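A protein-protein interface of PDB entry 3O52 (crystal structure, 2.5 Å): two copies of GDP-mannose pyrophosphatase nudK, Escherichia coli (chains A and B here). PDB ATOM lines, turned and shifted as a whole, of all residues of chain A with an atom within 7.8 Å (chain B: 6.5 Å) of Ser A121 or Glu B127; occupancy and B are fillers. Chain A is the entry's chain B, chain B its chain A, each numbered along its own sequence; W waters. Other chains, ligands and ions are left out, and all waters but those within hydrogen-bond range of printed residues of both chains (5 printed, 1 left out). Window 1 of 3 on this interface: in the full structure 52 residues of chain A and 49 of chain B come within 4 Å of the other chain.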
ATOM      1  N   TYR A  42      19.446  -1.557  -5.888  1.00  0.00           N
ATOM      2  CA  TYR A  42      19.510  -0.133  -5.641  1.00  0.00           C
ATOM      3  C   TYR A  42      20.031   0.130  -4.253  1.00  0.00           C
ATOM      4  O   TYR A  42      19.449  -0.301  -3.255  1.00  0.00           O
ATOM      5  CB  TYR A  42      18.105   0.453  -5.717  1.00  0.00           C
ATOM      6  CG  TYR A  42      17.992   1.961  -5.760  1.00  0.00           C
ATOM      7  CD1 TYR A  42      18.850   2.731  -6.555  1.00  0.00           C
ATOM      8  CD2 TYR A  42      16.977   2.611  -5.064  1.00  0.00           C
ATOM      9  CE1 TYR A  42      18.715   4.111  -6.632  1.00  0.00           C
ATOM     10  CE2 TYR A  42      16.840   4.004  -5.126  1.00  0.00           C
ATOM     11  CZ  TYR A  42      17.709   4.735  -5.916  1.00  0.00           C
ATOM     12  OH  TYR A  42      17.567   6.096  -5.998  1.00  0.00           O
ATOM     13  N   ALA A  69       7.841  10.188  -4.428  1.00  0.00           N
ATOM     14  CA  ALA A  69       7.685   8.760  -4.691  1.00  0.00           C
ATOM     15  C   ALA A  69       6.264   8.225  -4.484  1.00  0.00           C
ATOM     16  O   ALA A  69       5.871   7.276  -5.159  1.00  0.00           O
ATOM     17  CB  ALA A  69       8.673   7.951  -3.865  1.00  0.00           C
ATOM     18  N   THR A  70       5.522   8.817  -3.543  1.00  0.00           N
ATOM     19  CA  THR A  70       4.124   8.462  -3.314  1.00  0.00           C
ATOM     20  C   THR A  70       3.220   9.296  -4.231  1.00  0.00           C
ATOM     21  O   THR A  70       2.131   8.858  -4.632  1.00  0.00           O
ATOM     22  CB  THR A  70       3.709   8.661  -1.833  1.00  0.00           C
ATOM     23  OG1 THR A  70       3.649  10.062  -1.528  1.00  0.00           O
ATOM     24  CG2 THR A  70       4.687   7.966  -0.868  1.00  0.00           C
ATOM     25  N   ASN A  73       2.451   7.716  -7.396  1.00  0.00           N
ATOM     26  CA  ASN A  73       1.928   6.364  -7.135  1.00  0.00           C
ATOM     27  C   ASN A  73       0.765   6.358  -6.129  1.00  0.00           C
ATOM     28  O   ASN A  73       0.754   5.621  -5.128  1.00  0.00           O
ATOM     29  CB  ASN A  73       3.065   5.409  -6.734  1.00  0.00           C
ATOM     30  CG  ASN A  73       2.660   3.933  -6.768  1.00  0.00           C
ATOM     31  OD1 ASN A  73       1.661   3.571  -7.348  1.00  0.00           O
ATOM     32  ND2 ASN A  73       3.452   3.081  -6.130  1.00  0.00           N
ATOM     33  N   LEU A 118      15.840  -3.540  10.307  1.00  0.00           N
ATOM     34  CA  LEU A 118      15.096  -4.257   9.226  1.00  0.00           C
ATOM     35  C   LEU A 118      15.335  -3.714   7.837  1.00  0.00           C
ATOM     36  O   LEU A 118      15.421  -2.496   7.645  1.00  0.00           O
ATOM     37  CB  LEU A 118      13.581  -4.250   9.486  1.00  0.00           C
ATOM     38  CG  LEU A 118      13.151  -4.547  10.929  1.00  0.00           C
ATOM     39  CD1 LEU A 118      11.671  -4.421  11.086  1.00  0.00           C
ATOM     40  CD2 LEU A 118      13.660  -5.919  11.405  1.00  0.00           C
ATOM     41  N   TYR A 119      15.432  -4.643   6.879  1.00  0.00           N
ATOM     42  CA  TYR A 119      15.372  -4.355   5.440  1.00  0.00           C
ATOM     43  C   TYR A 119      13.937  -4.127   5.051  1.00  0.00           C
ATOM     44  O   TYR A 119      13.068  -5.005   5.272  1.00  0.00           O
ATOM     45  CB  TYR A 119      15.851  -5.566   4.656  1.00  0.00           C
ATOM     46  CG  TYR A 119      17.289  -5.957   4.920  1.00  0.00           C
ATOM     47  CD1 TYR A 119      17.572  -7.078   5.679  1.00  0.00           C
ATOM     48  CD2 TYR A 119      18.370  -5.201   4.397  1.00  0.00           C
ATOM     49  CE1 TYR A 119      18.867  -7.446   5.945  1.00  0.00           C
ATOM     50  CE2 TYR A 119      19.674  -5.553   4.670  1.00  0.00           C
ATOM     51  CZ  TYR A 119      19.909  -6.698   5.446  1.00  0.00           C
ATOM     52  OH  TYR A 119      21.186  -7.135   5.728  1.00  0.00           O
ATOM     53  N   MET A 120      13.654  -2.969   4.464  1.00  0.00           N
ATOM     54  CA  MET A 120      12.275  -2.636   4.114  1.00  0.00           C
ATOM     55  C   MET A 120      11.829  -3.212   2.795  1.00  0.00           C
ATOM     56  O   MET A 120      10.669  -3.594   2.648  1.00  0.00           O
ATOM     57  CB  MET A 120      12.057  -1.131   4.114  1.00  0.00           C
ATOM     58  CG  MET A 120      12.005  -0.513   5.524  1.00  0.00           C
ATOM     59  SD  MET A 120      10.889  -1.355   6.697  1.00  0.00           S
ATOM     60  CE  MET A 120      12.188  -1.893   7.730  1.00  0.00           C
ATOM     61  N   SER A 121      12.735  -3.276   1.828  1.00  0.00           N
ATOM     62  CA  SER A 121      12.376  -3.630   0.472  1.00  0.00           C
ATOM     63  C   SER A 121      13.516  -4.455  -0.137  1.00  0.00           C
ATOM     64  O   SER A 121      14.227  -4.020  -1.065  1.00  0.00           O
ATOM     65  CB  SER A 121      12.094  -2.342  -0.303  1.00  0.00           C
ATOM     66  OG  SER A 121      11.546  -2.626  -1.576  1.00  0.00           O
ATOM     67  N   PRO A 122      13.718  -5.654   0.419  1.00  0.00           N
ATOM     68  CA  PRO A 122      14.927  -6.457   0.185  1.00  0.00           C
ATOM     69  C   PRO A 122      15.002  -7.146  -1.190  1.00  0.00           C
ATOM     70  O   PRO A 122      16.036  -7.743  -1.556  1.00  0.00           O
ATOM     71  CB  PRO A 122      14.837  -7.513   1.297  1.00  0.00           C
ATOM     72  CG  PRO A 122      13.383  -7.666   1.544  1.00  0.00           C
ATOM     73  CD  PRO A 122      12.796  -6.305   1.375  1.00  0.00           C
ATOM     74  N   GLY A 123      13.918  -7.100  -1.942  1.00  0.00           N
ATOM     75  CA  GLY A 123      13.937  -7.691  -3.267  1.00  0.00           C
ATOM     76  C   GLY A 123      14.743  -6.918  -4.287  1.00  0.00           C
ATOM     77  O   GLY A 123      15.107  -7.472  -5.307  1.00  0.00           O
ATOM     78  N   GLY A 124      15.037  -5.652  -4.032  1.00  0.00           N
ATOM     79  CA  GLY A 124      15.928  -4.901  -4.908  1.00  0.00           C
ATOM     80  C   GLY A 124      16.520  -3.630  -4.326  1.00  0.00           C
ATOM     81  O   GLY A 124      17.196  -2.868  -5.033  1.00  0.00           O
ATOM     82  N   VAL A 125      16.265  -3.391  -3.043  1.00  0.00           N
ATOM     83  CA  VAL A 125      16.825  -2.234  -2.345  1.00  0.00           C
ATOM     84  C   VAL A 125      17.646  -2.801  -1.185  1.00  0.00           C
ATOM     85  O   VAL A 125      17.205  -3.704  -0.510  1.00  0.00           O
ATOM     86  CB  VAL A 125      15.701  -1.257  -1.827  1.00  0.00           C
ATOM     87  CG1 VAL A 125      16.272   0.103  -1.492  1.00  0.00           C
ATOM     88  CG2 VAL A 125      14.649  -1.083  -2.858  1.00  0.00           C
ATOM     89  N   THR A 126      18.858  -2.304  -0.992  1.00  0.00           N
ATOM     90  CA  THR A 126      19.725  -2.786   0.088  1.00  0.00           C
ATOM     91  C   THR A 126      19.303  -2.217   1.460  1.00  0.00           C
ATOM     92  O   THR A 126      19.717  -2.713   2.502  1.00  0.00           O
ATOM     93  CB  THR A 126      21.154  -2.322  -0.154  1.00  0.00           C
ATOM     94  OG1 THR A 126      21.123  -0.905  -0.317  1.00  0.00           O
ATOM     95  CG2 THR A 126      21.730  -2.934  -1.432  1.00  0.00           C
ATOM     96  N   GLU A 127      18.493  -1.172   1.453  1.00  0.00           N
ATOM     97  CA  GLU A 127      18.248  -0.349   2.650  1.00  0.00           C
ATOM     98  C   GLU A 127      17.941  -1.107   3.939  1.00  0.00           C
ATOM     99  O   GLU A 127      16.984  -1.894   4.001  1.00  0.00           O
ATOM    100  CB  GLU A 127      17.090   0.598   2.337  1.00  0.00           C
ATOM    101  CG  GLU A 127      16.755   1.623   3.393  1.00  0.00           C
ATOM    102  CD  GLU A 127      15.758   2.611   2.839  1.00  0.00           C
ATOM    103  OE1 GLU A 127      14.509   2.347   2.881  1.00  0.00           O
ATOM    104  OE2 GLU A 127      16.257   3.637   2.310  1.00  0.00           O
ATOM    105  N   LEU A 128      18.717  -0.807   4.975  1.00  0.00           N
ATOM    106  CA  LEU A 128      18.527  -1.348   6.317  1.00  0.00           C
ATOM    107  C   LEU A 128      18.111  -0.174   7.190  1.00  0.00           C
ATOM    108  O   LEU A 128      18.848   0.822   7.249  1.00  0.00           O
ATOM    109  CB  LEU A 128      19.840  -1.925   6.850  1.00  0.00           C
ATOM    110  CG  LEU A 128      19.856  -2.802   8.118  1.00  0.00           C
ATOM    111  CD1 LEU A 128      19.131  -4.118   7.882  1.00  0.00           C
ATOM    112  CD2 LEU A 128      21.310  -3.085   8.590  1.00  0.00           C
ATOM    113  N   ILE A 129      16.935  -0.270   7.837  1.00  0.00           N
ATOM    114  CA  ILE A 129      16.451   0.786   8.715  1.00  0.00           C
ATOM    115  C   ILE A 129      16.663   0.356  10.149  1.00  0.00           C
ATOM    116  O   ILE A 129      16.313  -0.763  10.529  1.00  0.00           O
ATOM    117  CB  ILE A 129      14.939   1.075   8.485  1.00  0.00           C
ATOM    118  CG1 ILE A 129      14.688   1.626   7.076  1.00  0.00           C
ATOM    119  CG2 ILE A 129      14.358   2.053   9.550  1.00  0.00           C
ATOM    120  CD1 ILE A 129      15.250   3.005   6.878  1.00  0.00           C
ATOM    121  N   ARG A 173      -0.185   5.192   6.279  1.00  0.00           N
ATOM    122  CA  ARG A 173      -0.067   4.100   5.308  1.00  0.00           C
ATOM    123  C   ARG A 173       1.401   3.860   4.969  1.00  0.00           C
ATOM    124  O   ARG A 173       1.763   3.491   3.850  1.00  0.00           O
ATOM    125  CB  ARG A 173      -0.896   4.421   4.068  1.00  0.00           C
ATOM    126  CG  ARG A 173      -0.730   5.865   3.599  1.00  0.00           C
ATOM    127  CD  ARG A 173      -1.155   6.073   2.160  1.00  0.00           C
ATOM    128  NE  ARG A 173      -2.601   5.960   1.964  1.00  0.00           N
ATOM    129  CZ  ARG A 173      -3.483   6.930   2.240  1.00  0.00           C
ATOM    130  NH1 ARG A 173      -3.060   8.091   2.763  1.00  0.00           N
ATOM    131  NH2 ARG A 173      -4.799   6.745   2.021  1.00  0.00           N
ATOM    132  N   GLY A 175       5.062   2.024   6.003  1.00  0.00           N
ATOM    133  CA  GLY A 175       5.520   0.779   6.631  1.00  0.00           C
ATOM    134  C   GLY A 175       6.172   0.909   7.991  1.00  0.00           C
ATOM    135  O   GLY A 175       5.736   0.266   8.966  1.00  0.00           O
ATOM    136  N   TYR B  42      12.748   5.528  -7.475  1.00  0.00           N
ATOM    137  CA  TYR B  42      12.839   4.180  -8.007  1.00  0.00           C
ATOM    138  C   TYR B  42      11.477   3.504  -8.062  1.00  0.00           C
ATOM    139  O   TYR B  42      10.780   3.402  -7.038  1.00  0.00           O
ATOM    140  CB  TYR B  42      13.766   3.357  -7.145  1.00  0.00           C
ATOM    141  CG  TYR B  42      14.255   2.057  -7.761  1.00  0.00           C
ATOM    142  CD1 TYR B  42      14.628   1.976  -9.100  1.00  0.00           C
ATOM    143  CD2 TYR B  42      14.395   0.911  -6.967  1.00  0.00           C
ATOM    144  CE1 TYR B  42      15.114   0.784  -9.637  1.00  0.00           C
ATOM    145  CE2 TYR B  42      14.882  -0.282  -7.488  1.00  0.00           C
ATOM    146  CZ  TYR B  42      15.231  -0.349  -8.818  1.00  0.00           C
ATOM    147  OH  TYR B  42      15.724  -1.549  -9.311  1.00  0.00           O
ATOM    148  N   ASP B  43      11.114   3.035  -9.249  1.00  0.00           N
ATOM    149  CA  ASP B  43       9.832   2.422  -9.459  1.00  0.00           C
ATOM    150  C   ASP B  43       9.989   0.974  -9.881  1.00  0.00           C
ATOM    151  O   ASP B  43      10.430   0.686 -10.981  1.00  0.00           O
ATOM    152  CB  ASP B  43       9.046   3.211 -10.528  1.00  0.00           C
ATOM    153  CG  ASP B  43       7.778   2.491 -10.988  1.00  0.00           C
ATOM    154  OD1 ASP B  43       7.394   1.477 -10.335  1.00  0.00           O
ATOM    155  OD2 ASP B  43       7.178   2.934 -12.007  1.00  0.00           O
ATOM    156  N   ARG B  44       9.627   0.065  -8.985  1.00  0.00           N
ATOM    157  CA  ARG B  44       9.574  -1.347  -9.319  1.00  0.00           C
ATOM    158  C   ARG B  44       8.128  -1.808  -9.303  1.00  0.00           C
ATOM    159  O   ARG B  44       7.856  -3.001  -9.240  1.00  0.00           O
ATOM    160  CB  ARG B  44      10.372  -2.222  -8.342  1.00  0.00           C
ATOM    161  CG  ARG B  44      11.344  -1.524  -7.397  1.00  0.00           C
ATOM    162  CD  ARG B  44      11.882  -2.501  -6.326  1.00  0.00           C
ATOM    163  NE  ARG B  44      12.935  -3.319  -6.907  1.00  0.00           N
ATOM    164  CZ  ARG B  44      12.922  -4.645  -7.018  1.00  0.00           C
ATOM    165  NH1 ARG B  44      11.913  -5.355  -6.552  1.00  0.00           N
ATOM    166  NH2 ARG B  44      13.948  -5.256  -7.582  1.00  0.00           N
ATOM    167  N   GLY B  45       7.183  -0.881  -9.376  1.00  0.00           N
ATOM    168  CA  GLY B  45       5.780  -1.274  -9.265  1.00  0.00           C
ATOM    169  C   GLY B  45       5.442  -1.639  -7.817  1.00  0.00           C
ATOM    170  O   GLY B  45       6.259  -1.470  -6.906  1.00  0.00           O
ATOM    171  N   ASN B  46       4.230  -2.138  -7.631  1.00  0.00           N
ATOM    172  CA  ASN B  46       3.679  -2.469  -6.345  1.00  0.00           C
ATOM    173  C   ASN B  46       3.663  -3.967  -6.086  1.00  0.00           C
ATOM    174  O   ASN B  46       3.867  -4.764  -6.985  1.00  0.00           O
ATOM    175  CB  ASN B  46       2.272  -1.875  -6.259  1.00  0.00           C
ATOM    176  CG  ASN B  46       2.292  -0.343  -6.272  1.00  0.00           C
ATOM    177  OD1 ASN B  46       3.250   0.275  -5.808  1.00  0.00           O
ATOM    178  ND2 ASN B  46       1.236   0.264  -6.796  1.00  0.00           N
ATOM    179  N   GLY B  47       3.439  -4.363  -4.843  1.00  0.00           N
ATOM    180  CA  GLY B  47       3.474  -5.786  -4.546  1.00  0.00           C
ATOM    181  C   GLY B  47       2.458  -6.125  -3.505  1.00  0.00           C
ATOM    182  O   GLY B  47       1.720  -5.257  -3.068  1.00  0.00           O
ATOM    183  N   ALA B  69      20.388  -8.064  -2.497  1.00  0.00           N
ATOM    184  CA  ALA B  69      20.496  -6.713  -1.955  1.00  0.00           C
ATOM    185  C   ALA B  69      20.824  -6.733  -0.460  1.00  0.00           C
ATOM    186  O   ALA B  69      21.400  -5.779   0.062  1.00  0.00           O
ATOM    187  CB  ALA B  69      19.253  -5.944  -2.205  1.00  0.00           C
ATOM    188  N   LEU B  87       5.747  -9.356  -6.639  1.00  0.00           N
ATOM    189  CA  LEU B  87       5.326  -8.196  -7.413  1.00  0.00           C
ATOM    190  C   LEU B  87       3.966  -8.481  -7.990  1.00  0.00           C
ATOM    191  O   LEU B  87       3.713  -9.595  -8.440  1.00  0.00           O
ATOM    192  CB  LEU B  87       6.310  -7.873  -8.530  1.00  0.00           C
ATOM    193  CG  LEU B  87       7.612  -7.332  -7.975  1.00  0.00           C
ATOM    194  CD1 LEU B  87       8.719  -7.390  -9.048  1.00  0.00           C
ATOM    195  CD2 LEU B  87       7.413  -5.933  -7.462  1.00  0.00           C
ATOM    196  N   LEU B 118       0.707  -0.194   2.273  1.00  0.00           N
ATOM    197  CA  LEU B 118       1.740   0.592   2.868  1.00  0.00           C
ATOM    198  C   LEU B 118       2.812   0.821   1.875  1.00  0.00           C
ATOM    199  O   LEU B 118       3.164  -0.098   1.119  1.00  0.00           O
ATOM    200  CB  LEU B 118       2.319  -0.118   4.086  1.00  0.00           C
ATOM    201  CG  LEU B 118       1.348  -0.611   5.195  1.00  0.00           C
ATOM    202  CD1 LEU B 118       2.104  -1.347   6.303  1.00  0.00           C
ATOM    203  CD2 LEU B 118       0.467   0.498   5.790  1.00  0.00           C
ATOM    204  N   TYR B 119       3.319   2.058   1.858  1.00  0.00           N
ATOM    205  CA  TYR B 119       4.587   2.372   1.198  1.00  0.00           C
ATOM    206  C   TYR B 119       5.698   1.886   2.114  1.00  0.00           C
ATOM    207  O   TYR B 119       5.795   2.314   3.281  1.00  0.00           O
ATOM    208  CB  TYR B 119       4.722   3.879   0.967  1.00  0.00           C
ATOM    209  CG  TYR B 119       3.705   4.440  -0.017  1.00  0.00           C
ATOM    210  CD1 TYR B 119       3.896   4.330  -1.384  1.00  0.00           C
ATOM    211  CD2 TYR B 119       2.549   5.081   0.438  1.00  0.00           C
ATOM    212  CE1 TYR B 119       2.971   4.841  -2.270  1.00  0.00           C
ATOM    213  CE2 TYR B 119       1.626   5.592  -0.426  1.00  0.00           C
ATOM    214  CZ  TYR B 119       1.834   5.469  -1.791  1.00  0.00           C
ATOM    215  OH  TYR B 119       0.885   5.999  -2.678  1.00  0.00           O
ATOM    216  N   MET B 120       6.522   0.968   1.631  1.00  0.00           N
ATOM    217  CA  MET B 120       7.562   0.439   2.492  1.00  0.00           C
ATOM    218  C   MET B 120       8.804   1.339   2.616  1.00  0.00           C
ATOM    219  O   MET B 120       9.492   1.300   3.651  1.00  0.00           O
ATOM    220  CB  MET B 120       7.920  -0.993   2.099  1.00  0.00           C
ATOM    221  CG  MET B 120       6.829  -2.004   2.431  1.00  0.00           C
ATOM    222  SD  MET B 120       6.366  -1.962   4.180  1.00  0.00           S
ATOM    223  CE  MET B 120       7.487  -3.211   4.844  1.00  0.00           C
ATOM    224  N   SER B 121       9.109   2.132   1.579  1.00  0.00           N
ATOM    225  CA  SER B 121      10.299   3.001   1.584  1.00  0.00           C
ATOM    226  C   SER B 121      10.079   4.282   0.759  1.00  0.00           C
ATOM    227  O   SER B 121      10.660   4.453  -0.328  1.00  0.00           O
ATOM    228  CB  SER B 121      11.461   2.220   1.007  1.00  0.00           C
ATOM    229  OG  SER B 121      12.686   2.920   1.167  1.00  0.00           O
ATOM    230  N   PRO B 122       9.244   5.192   1.269  1.00  0.00           N
ATOM    231  CA  PRO B 122       8.692   6.275   0.466  1.00  0.00           C
ATOM    232  C   PRO B 122       9.612   7.458   0.164  1.00  0.00           C
ATOM    233  O   PRO B 122       9.252   8.298  -0.658  1.00  0.00           O
ATOM    234  CB  PRO B 122       7.518   6.743   1.302  1.00  0.00           C
ATOM    235  CG  PRO B 122       7.966   6.489   2.705  1.00  0.00           C
ATOM    236  CD  PRO B 122       8.709   5.200   2.640  1.00  0.00           C
ATOM    237  N   VAL B 125      11.457   5.204  -3.119  1.00  0.00           N
ATOM    238  CA  VAL B 125      10.881   4.100  -3.887  1.00  0.00           C
ATOM    239  C   VAL B 125       9.391   4.308  -3.884  1.00  0.00           C
ATOM    240  O   VAL B 125       8.863   4.708  -2.862  1.00  0.00           O
ATOM    241  CB  VAL B 125      11.169   2.714  -3.248  1.00  0.00           C
ATOM    242  CG1 VAL B 125      10.652   1.580  -4.159  1.00  0.00           C
ATOM    243  CG2 VAL B 125      12.672   2.539  -2.942  1.00  0.00           C
ATOM    244  N   THR B 126       8.717   4.048  -5.015  1.00  0.00           N
ATOM    245  CA  THR B 126       7.260   4.153  -5.077  1.00  0.00           C
ATOM    246  C   THR B 126       6.522   2.968  -4.430  1.00  0.00           C
ATOM    247  O   THR B 126       5.314   3.030  -4.172  1.00  0.00           O
ATOM    248  CB  THR B 126       6.779   4.260  -6.521  1.00  0.00           C
ATOM    249  OG1 THR B 126       7.135   3.057  -7.213  1.00  0.00           O
ATOM    250  CG2 THR B 126       7.434   5.444  -7.222  1.00  0.00           C
ATOM    251  N   GLU B 127       7.243   1.884  -4.194  1.00  0.00           N
ATOM    252  CA  GLU B 127       6.626   0.607  -3.846  1.00  0.00           C
ATOM    253  C   GLU B 127       5.479   0.670  -2.838  1.00  0.00           C
ATOM    254  O   GLU B 127       5.699   1.001  -1.666  1.00  0.00           O
ATOM    255  CB  GLU B 127       7.683  -0.316  -3.273  1.00  0.00           C
ATOM    256  CG  GLU B 127       7.201  -1.729  -3.160  1.00  0.00           C
ATOM    257  CD  GLU B 127       8.358  -2.701  -3.111  1.00  0.00           C
ATOM    258  OE1 GLU B 127       8.922  -2.944  -1.994  1.00  0.00           O
ATOM    259  OE2 GLU B 127       8.683  -3.211  -4.206  1.00  0.00           O
ATOM    260  N   LEU B 128       4.276   0.314  -3.272  1.00  0.00           N
ATOM    261  CA  LEU B 128       3.159   0.081  -2.344  1.00  0.00           C
ATOM    262  C   LEU B 128       2.952  -1.434  -2.225  1.00  0.00           C
ATOM    263  O   LEU B 128       2.946  -2.151  -3.247  1.00  0.00           O
ATOM    264  CB  LEU B 128       1.911   0.779  -2.870  1.00  0.00           C
ATOM    265  CG  LEU B 128       0.600   1.033  -2.150  1.00  0.00           C
ATOM    266  CD1 LEU B 128       0.749   1.963  -0.964  1.00  0.00           C
ATOM    267  CD2 LEU B 128      -0.377   1.634  -3.154  1.00  0.00           C
ATOM    268  N   ILE B 129       2.851  -1.922  -0.988  1.00  0.00           N
ATOM    269  CA  ILE B 129       2.549  -3.334  -0.717  1.00  0.00           C
ATOM    270  C   ILE B 129       1.141  -3.499  -0.126  1.00  0.00           C
ATOM    271  O   ILE B 129       0.757  -2.791   0.814  1.00  0.00           O
ATOM    272  CB  ILE B 129       3.574  -3.966   0.237  1.00  0.00           C
ATOM    273  CG1 ILE B 129       4.998  -3.839  -0.314  1.00  0.00           C
ATOM    274  CG2 ILE B 129       3.189  -5.409   0.617  1.00  0.00           C
ATOM    275  CD1 ILE B 129       5.363  -4.829  -1.341  1.00  0.00           C
ATOM    276  N   ASP B 174      13.066  -8.587   8.384  1.00  0.00           N
ATOM    277  CA  ASP B 174      12.415  -8.120   7.184  1.00  0.00           C
ATOM    278  C   ASP B 174      11.207  -7.289   7.582  1.00  0.00           C
ATOM    279  O   ASP B 174      10.294  -7.790   8.231  1.00  0.00           O
ATOM    280  CB  ASP B 174      11.984  -9.284   6.319  1.00  0.00           C
ATOM    281  CG  ASP B 174      11.165  -8.839   5.179  1.00  0.00           C
ATOM    282  OD1 ASP B 174       9.970  -9.232   5.128  1.00  0.00           O
ATOM    283  OD2 ASP B 174      11.703  -8.059   4.345  1.00  0.00           O
ATOM    284  N   GLY B 175      11.203  -6.036   7.156  1.00  0.00           N
ATOM    285  CA  GLY B 175      10.190  -5.081   7.579  1.00  0.00           C
ATOM    286  C   GLY B 175       8.772  -5.582   7.500  1.00  0.00           C
ATOM    287  O   GLY B 175       8.023  -5.519   8.504  1.00  0.00           O
HETATM  288  O   HOH W   1       8.740  -4.409   0.885  1.00  0.00           O
HETATM  289  O   HOH W   2       8.154   3.165   5.607  1.00  0.00           O
HETATM  290  O   HOH W   3       9.898  10.368  -2.114  1.00  0.00           O
HETATM  291  O   HOH W   4       9.982  -5.889   3.860  1.00  0.00           O
HETATM  292  O   HOH W   5      17.550  -8.964  -3.345  1.00  0.00           O
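Ala A69 touches Val B125.
Thr B126 touches Ala A69 (CG2 to O, 3.2 Å).
Thr A70 touches Pro B122.
CB of Leu A118 touches N of Gly B175, at 3.8 Å.
Met A120 touches Gly B175 (CE to CA, 3.8 Å).
Ala B69 touches Pro A122.
Pro A122 touches Asp B174 (CG to OD2, 3.3 Å).
O of Val A125 touches CB of Ala B69, at 3.5 Å.
Thr A126 touches Ala B69.
Arg A173 touches Leu B118 (O to CA, 3.1 Å).
Of chain B, only Glu B127 comes within 4 Å of Ser A121.
Leu A128 touches none of the printed residues of chain B.
Printed residues of chain A within 4 Å of Leu B118: Arg A173 and Gly A175.
Of the printed residues of chain A, Ser B121 touches Glu A127 (2.6 Å).
Glu B127 touches one residue of chain A.
The nearest printed residue of chain B that does not touch Ser A121 is Arg B44 (4.8 Å).
Hydrophobic or aromatic side chains of chain A within 4 Å of the printed part of chain B: Tyr A42, Ala A69, Leu A118, Met A120 and Pro A122.
Printed residues of chain B that touch a printed residue of chain A: Tyr B42, Arg B44, Asn B46, Ala B69, Leu B118, Tyr B119, Met B120, Ser B121, Pro B122, Val B125, Thr B126, Glu B127, Asp B174 and Gly B175.
Hydrophobic or aromatic side chains of chain B that line the printed part of chain A: Tyr B42, Ala B69, Leu B118, Tyr B119, Met B120 and Pro B122.
Ala A69 touches Pro B122, and with the chains exchanged Pro A122 touches Ala B69.
Tyr A119 touches Gly B175, and with the chains exchanged Gly A175 touches Tyr B119.
Met B120 touches its own counterpart, Met A120.
Met A120 touches Gly B175, and with the chains exchanged Gly A175 touches Met B120.
Water W3 bridges O of Pro B122 (2.6 Å) and N of Ala A69 (3.1 Å).
Water W5 lies within hydrogen-bond range of O of Pro A122 (2.6 Å), N of Ala B69 (3.1 Å) and O of Gly A123 (3.5 Å).
Water W4 bridges O of Met A120 (2.7 Å) and OD2 of Asp B174 (2.8 Å).
Water W1 bridges O of Met A120 and OE1 of Glu B127.
Water W2 lies within hydrogen-bond range of the backbone carbonyl oxygen of Met B120 (3.0 Å), the backbone NH of Gly A175 (3.3 Å) and the backbone carbonyl oxygen of Tyr B119 (3.4 Å).
The side-chain amide oxygen of Asn B46 lies within hydrogen-bond range of the backbone NH of Leu B128.
The backbone carbonyl oxygen of Leu B118 lies within hydrogen-bond range of the backbone NH of Ile B129 (2.8 Å).
The backbone NH (N) of Met B120 lies within hydrogen-bond range of the backbone carbonyl oxygen (O) of Glu B127.
The backbone NH of Tyr A42 is in hydrogen-bond range of the backbone carbonyl oxygen of Gly A124 (2.7 Å).
The backbone carbonyl oxygen (O) of Tyr A42 sits at hydrogen-bond distance from the backbone NH (N) of Thr A126, 3.1 Å away.
O of Leu A118 sits at hydrogen-bond distance from N of Ile A129.
O of Gly A123 is in hydrogen-bond range of NH2 of Arg B44.
The side-chain amide nitrogen of Asn A73 lies within hydrogen-bond range of the side-chain amide oxygen of Asn B46, 2.8 Å away.
The side-chain hydroxyl (OH) of Tyr B119 sits at hydrogen-bond distance from the backbone carbonyl oxygen (O) of Asn A73, 2.5 Å away.
N of Tyr B119 lies within hydrogen-bond range of O of Arg A173, 2.9 Å away.
O of Tyr B119 is in hydrogen-bond range of N of Gly A175 (2.8 Å).
OG of Ser B121 sits at hydrogen-bond distance from OE1 of Glu A127, 2.6 Å away.
ND2 of Asn A73 is in hydrogen-bond range of O of Thr B126 (2.7 Å).
OE1 of Glu B127 lies within hydrogen-bond range of OG of Ser A121 (2.7 Å).
N of Gly B175 sits at hydrogen-bond distance from O of Tyr A119 (2.8 Å).
OD2 of Asp B174 lies close to O of Tyr A119, 3.5 Å away.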
